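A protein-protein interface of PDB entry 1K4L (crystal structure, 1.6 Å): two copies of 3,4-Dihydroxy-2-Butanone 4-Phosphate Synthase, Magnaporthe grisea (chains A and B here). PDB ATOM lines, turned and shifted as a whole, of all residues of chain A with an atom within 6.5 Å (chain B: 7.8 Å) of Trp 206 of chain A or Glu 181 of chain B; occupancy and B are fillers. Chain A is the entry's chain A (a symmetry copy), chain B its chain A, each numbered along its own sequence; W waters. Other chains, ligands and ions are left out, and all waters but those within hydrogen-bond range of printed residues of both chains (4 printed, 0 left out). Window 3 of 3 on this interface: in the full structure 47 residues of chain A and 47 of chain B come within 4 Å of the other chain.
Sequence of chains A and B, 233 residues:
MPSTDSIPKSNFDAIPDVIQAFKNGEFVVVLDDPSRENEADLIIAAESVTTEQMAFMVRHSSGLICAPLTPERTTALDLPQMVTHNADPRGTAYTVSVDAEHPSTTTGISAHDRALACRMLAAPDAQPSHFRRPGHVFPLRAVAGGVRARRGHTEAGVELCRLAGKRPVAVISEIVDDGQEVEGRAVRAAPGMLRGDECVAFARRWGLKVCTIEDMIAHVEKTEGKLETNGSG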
ATOM      1  N   PHE A  56      -4.124   5.856 -15.025  1.00  0.00           N
ATOM      2  CA  PHE A  56      -4.246   4.797 -14.042  1.00  0.00           C
ATOM      3  C   PHE A  56      -4.203   5.373 -12.634  1.00  0.00           C
ATOM      4  O   PHE A  56      -4.958   4.981 -11.718  1.00  0.00           O
ATOM      5  CB  PHE A  56      -3.138   3.695 -14.186  1.00  0.00           C
ATOM      6  CG  PHE A  56      -3.225   2.568 -13.188  1.00  0.00           C
ATOM      7  CD1 PHE A  56      -4.008   1.430 -13.460  1.00  0.00           C
ATOM      8  CD2 PHE A  56      -2.496   2.619 -12.000  1.00  0.00           C
ATOM      9  CE1 PHE A  56      -4.066   0.372 -12.553  1.00  0.00           C
ATOM     10  CE2 PHE A  56      -2.580   1.571 -11.079  1.00  0.00           C
ATOM     11  CZ  PHE A  56      -3.358   0.437 -11.352  1.00  0.00           C
ATOM     12  N   HIS A  60      -7.267   5.079  -9.833  1.00  0.00           N
ATOM     13  CA  HIS A  60      -7.178   4.339  -8.588  1.00  0.00           C
ATOM     14  C   HIS A  60      -6.900   5.111  -7.286  1.00  0.00           C
ATOM     15  O   HIS A  60      -6.864   4.549  -6.176  1.00  0.00           O
ATOM     16  CB  HIS A  60      -6.209   3.143  -8.758  1.00  0.00           C
ATOM     17  CG  HIS A  60      -6.685   2.205  -9.858  1.00  0.00           C
ATOM     18  ND1 HIS A  60      -7.655   1.247  -9.592  1.00  0.00           N
ATOM     19  CD2 HIS A  60      -6.358   2.103 -11.188  1.00  0.00           C
ATOM     20  CE1 HIS A  60      -7.899   0.602 -10.735  1.00  0.00           C
ATOM     21  NE2 HIS A  60      -7.163   1.103 -11.714  1.00  0.00           N
ATOM     22  N   ALA A 201      -2.663  -6.670  -1.729  1.00  0.00           N
ATOM     23  CA  ALA A 201      -3.406  -7.314  -2.788  1.00  0.00           C
ATOM     24  C   ALA A 201      -3.541  -6.450  -4.015  1.00  0.00           C
ATOM     25  O   ALA A 201      -3.482  -6.943  -5.157  1.00  0.00           O
ATOM     26  CB  ALA A 201      -4.789  -7.753  -2.327  1.00  0.00           C
ATOM     27  N   PHE A 202      -3.754  -5.128  -3.758  1.00  0.00           N
ATOM     28  CA  PHE A 202      -3.889  -4.155  -4.835  1.00  0.00           C
ATOM     29  C   PHE A 202      -2.570  -4.176  -5.648  1.00  0.00           C
ATOM     30  O   PHE A 202      -2.548  -4.208  -6.888  1.00  0.00           O
ATOM     31  CB  PHE A 202      -4.123  -2.746  -4.232  1.00  0.00           C
ATOM     32  CG  PHE A 202      -4.079  -1.668  -5.291  1.00  0.00           C
ATOM     33  CD1 PHE A 202      -5.214  -1.295  -6.030  1.00  0.00           C
ATOM     34  CD2 PHE A 202      -2.871  -1.021  -5.590  1.00  0.00           C
ATOM     35  CE1 PHE A 202      -5.178  -0.319  -7.030  1.00  0.00           C
ATOM     36  CE2 PHE A 202      -2.804  -0.041  -6.590  1.00  0.00           C
ATOM     37  CZ  PHE A 202      -3.957   0.321  -7.297  1.00  0.00           C
ATOM     38  N   ALA A 203      -1.468  -4.165  -4.898  1.00  0.00           N
ATOM     39  CA  ALA A 203      -0.183  -4.172  -5.583  1.00  0.00           C
ATOM     40  C   ALA A 203      -0.018  -5.437  -6.420  1.00  0.00           C
ATOM     41  O   ALA A 203       0.387  -5.374  -7.597  1.00  0.00           O
ATOM     42  CB  ALA A 203       0.985  -4.017  -4.606  1.00  0.00           C
ATOM     43  N   ARG A 204      -0.332  -6.575  -5.800  1.00  0.00           N
ATOM     44  CA  ARG A 204      -0.189  -7.831  -6.554  1.00  0.00           C
ATOM     45  C   ARG A 204      -1.027  -7.847  -7.808  1.00  0.00           C
ATOM     46  O   ARG A 204      -0.629  -8.333  -8.911  1.00  0.00           O
ATOM     47  CB  ARG A 204      -0.409  -9.061  -5.702  1.00  0.00           C
ATOM     48  CG  ARG A 204       0.345  -9.078  -4.368  1.00  0.00           C
ATOM     49  CD  ARG A 204       1.802  -8.710  -4.595  1.00  0.00           C
ATOM     50  NE  ARG A 204       2.632  -8.918  -3.414  1.00  0.00           N
ATOM     51  CZ  ARG A 204       3.859  -8.417  -3.298  1.00  0.00           C
ATOM     52  NH1 ARG A 204       4.366  -7.687  -4.303  1.00  0.00           N
ATOM     53  NH2 ARG A 204       4.553  -8.682  -2.176  1.00  0.00           N
ATOM     54  N   ARG A 205      -2.236  -7.268  -7.695  1.00  0.00           N
ATOM     55  CA  ARG A 205      -3.134  -7.228  -8.834  1.00  0.00           C
ATOM     56  C   ARG A 205      -2.591  -6.501 -10.058  1.00  0.00           C
ATOM     57  O   ARG A 205      -2.843  -6.862 -11.205  1.00  0.00           O
ATOM     58  CB  ARG A 205      -4.458  -6.561  -8.365  1.00  0.00           C
ATOM     59  CG  ARG A 205      -5.498  -6.311  -9.450  1.00  0.00           C
ATOM     60  CD  ARG A 205      -6.794  -5.717  -8.871  1.00  0.00           C
ATOM     61  NE  ARG A 205      -7.122  -6.439  -7.641  1.00  0.00           N
ATOM     62  CZ  ARG A 205      -7.285  -5.896  -6.419  1.00  0.00           C
ATOM     63  NH1 ARG A 205      -7.228  -4.581  -6.216  1.00  0.00           N
ATOM     64  NH2 ARG A 205      -7.524  -6.698  -5.368  1.00  0.00           N
ATOM     65  N   TRP A 206      -1.852  -5.400  -9.810  1.00  0.00           N
ATOM     66  CA  TRP A 206      -1.338  -4.586 -10.885  1.00  0.00           C
ATOM     67  C   TRP A 206       0.163  -4.784 -11.155  1.00  0.00           C
ATOM     68  O   TRP A 206       0.756  -3.940 -11.819  1.00  0.00           O
ATOM     69  CB  TRP A 206      -1.637  -3.106 -10.508  1.00  0.00           C
ATOM     70  CG  TRP A 206      -3.107  -2.912 -10.389  1.00  0.00           C
ATOM     71  CD1 TRP A 206      -3.812  -2.633  -9.247  1.00  0.00           C
ATOM     72  CD2 TRP A 206      -4.040  -2.990 -11.459  1.00  0.00           C
ATOM     73  NE1 TRP A 206      -5.153  -2.512  -9.576  1.00  0.00           N
ATOM     74  CE2 TRP A 206      -5.338  -2.720 -10.912  1.00  0.00           C
ATOM     75  CE3 TRP A 206      -3.915  -3.220 -12.828  1.00  0.00           C
ATOM     76  CZ2 TRP A 206      -6.501  -2.737 -11.683  1.00  0.00           C
ATOM     77  CZ3 TRP A 206      -5.065  -3.206 -13.616  1.00  0.00           C
ATOM     78  CH2 TRP A 206      -6.350  -2.973 -13.037  1.00  0.00           C
ATOM     79  N   GLY A 207       0.755  -5.829 -10.595  1.00  0.00           N
ATOM     80  CA  GLY A 207       2.185  -6.110 -10.855  1.00  0.00           C
ATOM     81  C   GLY A 207       3.175  -5.113 -10.266  1.00  0.00           C
ATOM     82  O   GLY A 207       4.236  -4.831 -10.836  1.00  0.00           O
ATOM     83  N   LEU A 208       2.823  -4.579  -9.106  1.00  0.00           N
ATOM     84  CA  LEU A 208       3.668  -3.562  -8.459  1.00  0.00           C
ATOM     85  C   LEU A 208       4.319  -4.061  -7.218  1.00  0.00           C
ATOM     86  O   LEU A 208       3.813  -4.965  -6.565  1.00  0.00           O
ATOM     87  CB  LEU A 208       2.846  -2.302  -8.049  1.00  0.00           C
ATOM     88  CG  LEU A 208       1.970  -1.818  -9.193  1.00  0.00           C
ATOM     89  CD1 LEU A 208       1.037  -0.682  -8.737  1.00  0.00           C
ATOM     90  CD2 LEU A 208       2.772  -1.372 -10.429  1.00  0.00           C
ATOM     91  N   ASP B 178     -11.489   7.967 -18.263  1.00  0.00           N
ATOM     92  CA  ASP B 178     -10.400   7.173 -17.721  1.00  0.00           C
ATOM     93  C   ASP B 178      -9.871   6.111 -18.684  1.00  0.00           C
ATOM     94  O   ASP B 178      -9.083   5.259 -18.270  1.00  0.00           O
ATOM     95  CB  ASP B 178     -10.722   6.494 -16.391  1.00  0.00           C
ATOM     96  CG  ASP B 178     -12.061   5.823 -16.530  1.00  0.00           C
ATOM     97  OD1 ASP B 178     -12.540   5.530 -17.623  1.00  0.00           O
ATOM     98  OD2 ASP B 178     -12.701   5.724 -15.389  1.00  0.00           O
ATOM     99  N   GLY B 179     -10.314   6.179 -19.929  1.00  0.00           N
ATOM    100  CA  GLY B 179      -9.874   5.231 -20.945  1.00  0.00           C
ATOM    101  C   GLY B 179     -10.212   3.781 -20.570  1.00  0.00           C
ATOM    102  O   GLY B 179     -11.153   3.500 -19.842  1.00  0.00           O
ATOM    103  N   GLN B 180      -9.423   2.819 -21.019  1.00  0.00           N
ATOM    104  CA  GLN B 180      -9.766   1.456 -20.639  1.00  0.00           C
ATOM    105  C   GLN B 180      -8.725   0.778 -19.778  1.00  0.00           C
ATOM    106  O   GLN B 180      -7.544   1.088 -19.894  1.00  0.00           O
ATOM    107  CB  GLN B 180     -10.040   0.584 -21.882  1.00  0.00           C
ATOM    108  CG  GLN B 180     -11.218   1.103 -22.737  1.00  0.00           C
ATOM    109  CD  GLN B 180     -10.758   2.139 -23.748  1.00  0.00           C
ATOM    110  OE1 GLN B 180     -11.408   3.181 -23.948  1.00  0.00           O
ATOM    111  NE2 GLN B 180      -9.611   1.885 -24.375  1.00  0.00           N
ATOM    112  N   GLU B 181      -9.188  -0.138 -18.951  1.00  0.00           N
ATOM    113  CA  GLU B 181      -8.322  -0.951 -18.112  1.00  0.00           C
ATOM    114  C   GLU B 181      -7.430  -1.811 -19.030  1.00  0.00           C
ATOM    115  O   GLU B 181      -7.843  -2.135 -20.132  1.00  0.00           O
ATOM    116  CB  GLU B 181      -9.141  -2.005 -17.337  1.00  0.00           C
ATOM    117  CG  GLU B 181      -8.226  -2.978 -16.562  1.00  0.00           C
ATOM    118  CD  GLU B 181      -8.962  -4.043 -15.794  1.00  0.00           C
ATOM    119  OE1 GLU B 181     -10.160  -4.203 -15.856  1.00  0.00           O
ATOM    120  OE2 GLU B 181      -8.190  -4.804 -15.064  1.00  0.00           O
ATOM    121  N   VAL B 182      -6.237  -2.143 -18.549  1.00  0.00           N
ATOM    122  CA  VAL B 182      -5.239  -2.998 -19.220  1.00  0.00           C
ATOM    123  C   VAL B 182      -4.921  -4.030 -18.160  1.00  0.00           C
ATOM    124  O   VAL B 182      -4.267  -3.754 -17.143  1.00  0.00           O
ATOM    125  CB  VAL B 182      -3.995  -2.204 -19.667  1.00  0.00           C
ATOM    126  CG1 VAL B 182      -2.969  -3.188 -20.289  1.00  0.00           C
ATOM    127  CG2 VAL B 182      -4.447  -1.135 -20.671  1.00  0.00           C
ATOM    128  N   GLU B 183      -5.527  -5.220 -18.383  1.00  0.00           N
ATOM    129  CA  GLU B 183      -5.463  -6.312 -17.442  1.00  0.00           C
ATOM    130  C   GLU B 183      -4.090  -6.462 -16.904  1.00  0.00           C
ATOM    131  O   GLU B 183      -3.167  -6.557 -17.715  1.00  0.00           O
ATOM    132  CB  GLU B 183      -5.994  -7.640 -18.051  1.00  0.00           C
ATOM    133  CG  GLU B 183      -5.743  -8.861 -17.134  1.00  0.00           C
ATOM    134  CD  GLU B 183      -6.527  -8.736 -15.851  1.00  0.00           C
ATOM    135  OE1 GLU B 183      -7.312  -7.833 -15.623  1.00  0.00           O
ATOM    136  OE2 GLU B 183      -6.244  -9.659 -14.978  1.00  0.00           O
ATOM    137  N   GLY B 184      -3.955  -6.449 -15.611  1.00  0.00           N
ATOM    138  CA  GLY B 184      -2.628  -6.625 -14.997  1.00  0.00           C
ATOM    139  C   GLY B 184      -1.537  -5.553 -15.195  1.00  0.00           C
ATOM    140  O   GLY B 184      -0.410  -5.744 -14.726  1.00  0.00           O
ATOM    141  N   ARG B 185      -1.866  -4.429 -15.829  1.00  0.00           N
ATOM    142  CA  ARG B 185      -0.864  -3.394 -16.019  1.00  0.00           C
ATOM    143  C   ARG B 185      -1.309  -2.056 -15.427  1.00  0.00           C
ATOM    144  O   ARG B 185      -2.473  -1.674 -15.620  1.00  0.00           O
ATOM    145  CB  ARG B 185      -0.595  -3.132 -17.486  1.00  0.00           C
ATOM    146  CG  ARG B 185      -0.132  -4.358 -18.263  1.00  0.00           C
ATOM    147  CD  ARG B 185       1.235  -4.903 -17.906  1.00  0.00           C
ATOM    148  NE  ARG B 185       1.526  -6.071 -18.732  1.00  0.00           N
ATOM    149  CZ  ARG B 185       2.401  -7.010 -18.373  1.00  0.00           C
ATOM    150  NH1 ARG B 185       3.084  -6.920 -17.244  1.00  0.00           N
ATOM    151  NH2 ARG B 185       2.640  -8.068 -19.179  1.00  0.00           N
ATOM    152  N   ALA B 186      -0.349  -1.322 -14.827  1.00  0.00           N
ATOM    153  CA  ALA B 186      -0.584  -0.023 -14.208  1.00  0.00           C
ATOM    154  C   ALA B 186      -0.683   1.109 -15.179  1.00  0.00           C
ATOM    155  O   ALA B 186       0.000   2.114 -15.028  1.00  0.00           O
ATOM    156  CB  ALA B 186       0.245   0.243 -12.971  1.00  0.00           C
ATOM    157  N   VAL B 187      -1.557   0.945 -16.164  1.00  0.00           N
ATOM    158  CA  VAL B 187      -1.806   1.961 -17.158  1.00  0.00           C
ATOM    159  C   VAL B 187      -3.274   1.909 -17.601  1.00  0.00           C
ATOM    160  O   VAL B 187      -3.908   0.887 -17.383  1.00  0.00           O
ATOM    161  CB  VAL B 187      -0.932   1.812 -18.413  1.00  0.00           C
ATOM    162  CG1 VAL B 187       0.569   1.994 -18.050  1.00  0.00           C
ATOM    163  CG2 VAL B 187      -1.274   0.452 -19.065  1.00  0.00           C
ATOM    164  N   ARG B 188      -3.771   2.983 -18.236  1.00  0.00           N
ATOM    165  CA  ARG B 188      -5.125   3.002 -18.802  1.00  0.00           C
ATOM    166  C   ARG B 188      -4.949   3.427 -20.229  1.00  0.00           C
ATOM    167  O   ARG B 188      -4.279   4.416 -20.495  1.00  0.00           O
ATOM    168  CB  ARG B 188      -6.212   3.866 -18.146  1.00  0.00           C
ATOM    169  CG  ARG B 188      -6.156   3.764 -16.647  1.00  0.00           C
ATOM    170  CD  ARG B 188      -7.203   2.842 -16.083  1.00  0.00           C
ATOM    171  NE  ARG B 188      -8.518   3.058 -16.693  1.00  0.00           N
ATOM    172  CZ  ARG B 188      -9.559   2.296 -16.351  1.00  0.00           C
ATOM    173  NH1 ARG B 188      -9.476   1.323 -15.437  1.00  0.00           N
ATOM    174  NH2 ARG B 188     -10.725   2.533 -16.921  1.00  0.00           N
ATOM    175  N   ALA B 189      -5.520   2.709 -21.188  1.00  0.00           N
ATOM    176  CA  ALA B 189      -5.343   3.101 -22.560  1.00  0.00           C
ATOM    177  C   ALA B 189      -6.371   4.114 -23.023  1.00  0.00           C
ATOM    178  O   ALA B 189      -7.563   4.038 -22.665  1.00  0.00           O
ATOM    179  CB  ALA B 189      -5.510   1.828 -23.380  1.00  0.00           C
HETATM  180  O   HOH W   1       2.094  -2.860 -13.915  1.00  0.00           O
HETATM  181  O   HOH W   2      -4.647  -8.787 -12.334  1.00  0.00           O
HETATM  182  O   HOH W   3      -5.546  -6.451 -13.280  1.00  0.00           O
HETATM  183  O   HOH W   4      -7.260  -0.051 -14.209  1.00  0.00           O
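The guanidinium group of Arg 188 of chain B is in hydrogen-bond range of the backbone carbonyl oxygen of Gly 179 of chain B (3.1 Å). The guanidinium group (NH2) of Arg 188 of chain B is in salt-bridge range of the side-chain carboxylate (OD1) of Asp 178 of chain B, at 3.6 Å. The backbone carbonyl oxygen of Ala 203 of chain A is in hydrogen-bond range of the backbone NH of Leu 208 of chain A, 3.0 Å away.
Water W1 lies within hydrogen-bond range of the backbone carbonyl oxygen (O) of Trp 206 of chain A (2.7 Å) and the backbone NH (N) of Ala 186 of chain B (3.0 Å). Water W4 lies within hydrogen-bond range of NE2 of His 60 of chain A (2.8 Å) and NH1 of Arg 188 of chain B (2.9 Å). Water W3 lies within hydrogen-bond range of the backbone NH of Gly 184 of chain B (2.8 Å), the side-chain carboxylate of Glu 183 of chain B (3.2 Å) and the backbone carbonyl oxygen of Arg 205 of chain A (3.4 Å). Water W2 bridges the backbone carbonyl oxygen (O) of Arg 205 of chain A (2.9 Å) and the side-chain carboxylate (OE2) of Glu 183 of chain B (3.2 Å).
Ala 201 of chain A touches none of the printed residues of chain B. Trp 206 of chain A touches four residues of chain B. Of the printed residues of chain B, Leu 208 of chain A touches Ala 186 (3.9 Å). Gly 179 of chain B touches none of the printed residues of chain A. Of chain A, only Trp 206 (3.3 Å) comes within 4 Å of Glu 181 of chain B. Printed residues of chain A within 4 Å of Arg 185 of chain B: Trp 206. Of the printed residues of chain A, Val 187 of chain B touches Phe 56 (3.7 Å). The nearest printed residue of chain A that does not touch Glu 181 of chain B is Arg 205 of chain A (6.4 Å). The nearest printed residue of chain A that does not touch Val 182 of chain B is Phe 56 of chain A (6.2 Å).
No position is printed for both chains.
Hydrophobic or aromatic side chains of chain B that line the printed part of chain A: Ala 186. Of the 10 printed residues of chain A, 4 touch a printed residue of chain B. Along chain A the printed residues that touch a printed residue of chain B span positions 56 to 208. Among the printed residues, no Asp or Glu carboxylate lies within 4 Å of a Lys or Arg side-chain nitrogen of the other chain.
Phe 56 of chain A touches Ala 186 of chain B (CG to C, 3.5 Å). Val 187 of chain B touches Phe 56 of chain A. N of Phe 56 of chain A touches CG of Arg 188 of chain B, at 3.3 Å. O of Arg 205 of chain A touches CA of Gly 184 of chain B (3.8 Å). Trp 206 of chain A touches Glu 181 of chain B (CH2 to OE2, 3.3 Å). Trp 206 of chain A touches Val 182 of chain B (CZ3 to O, 3.7 Å). Trp 206 of chain A touches Gly 184 of chain B (O to O, 3.6 Å). CE3 of Trp 206 of chain A touches O of Arg 185 of chain B (3.5 Å). Leu 208 of chain A touches Ala 186 of chain B (CD2 to CB, 3.9 Å).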
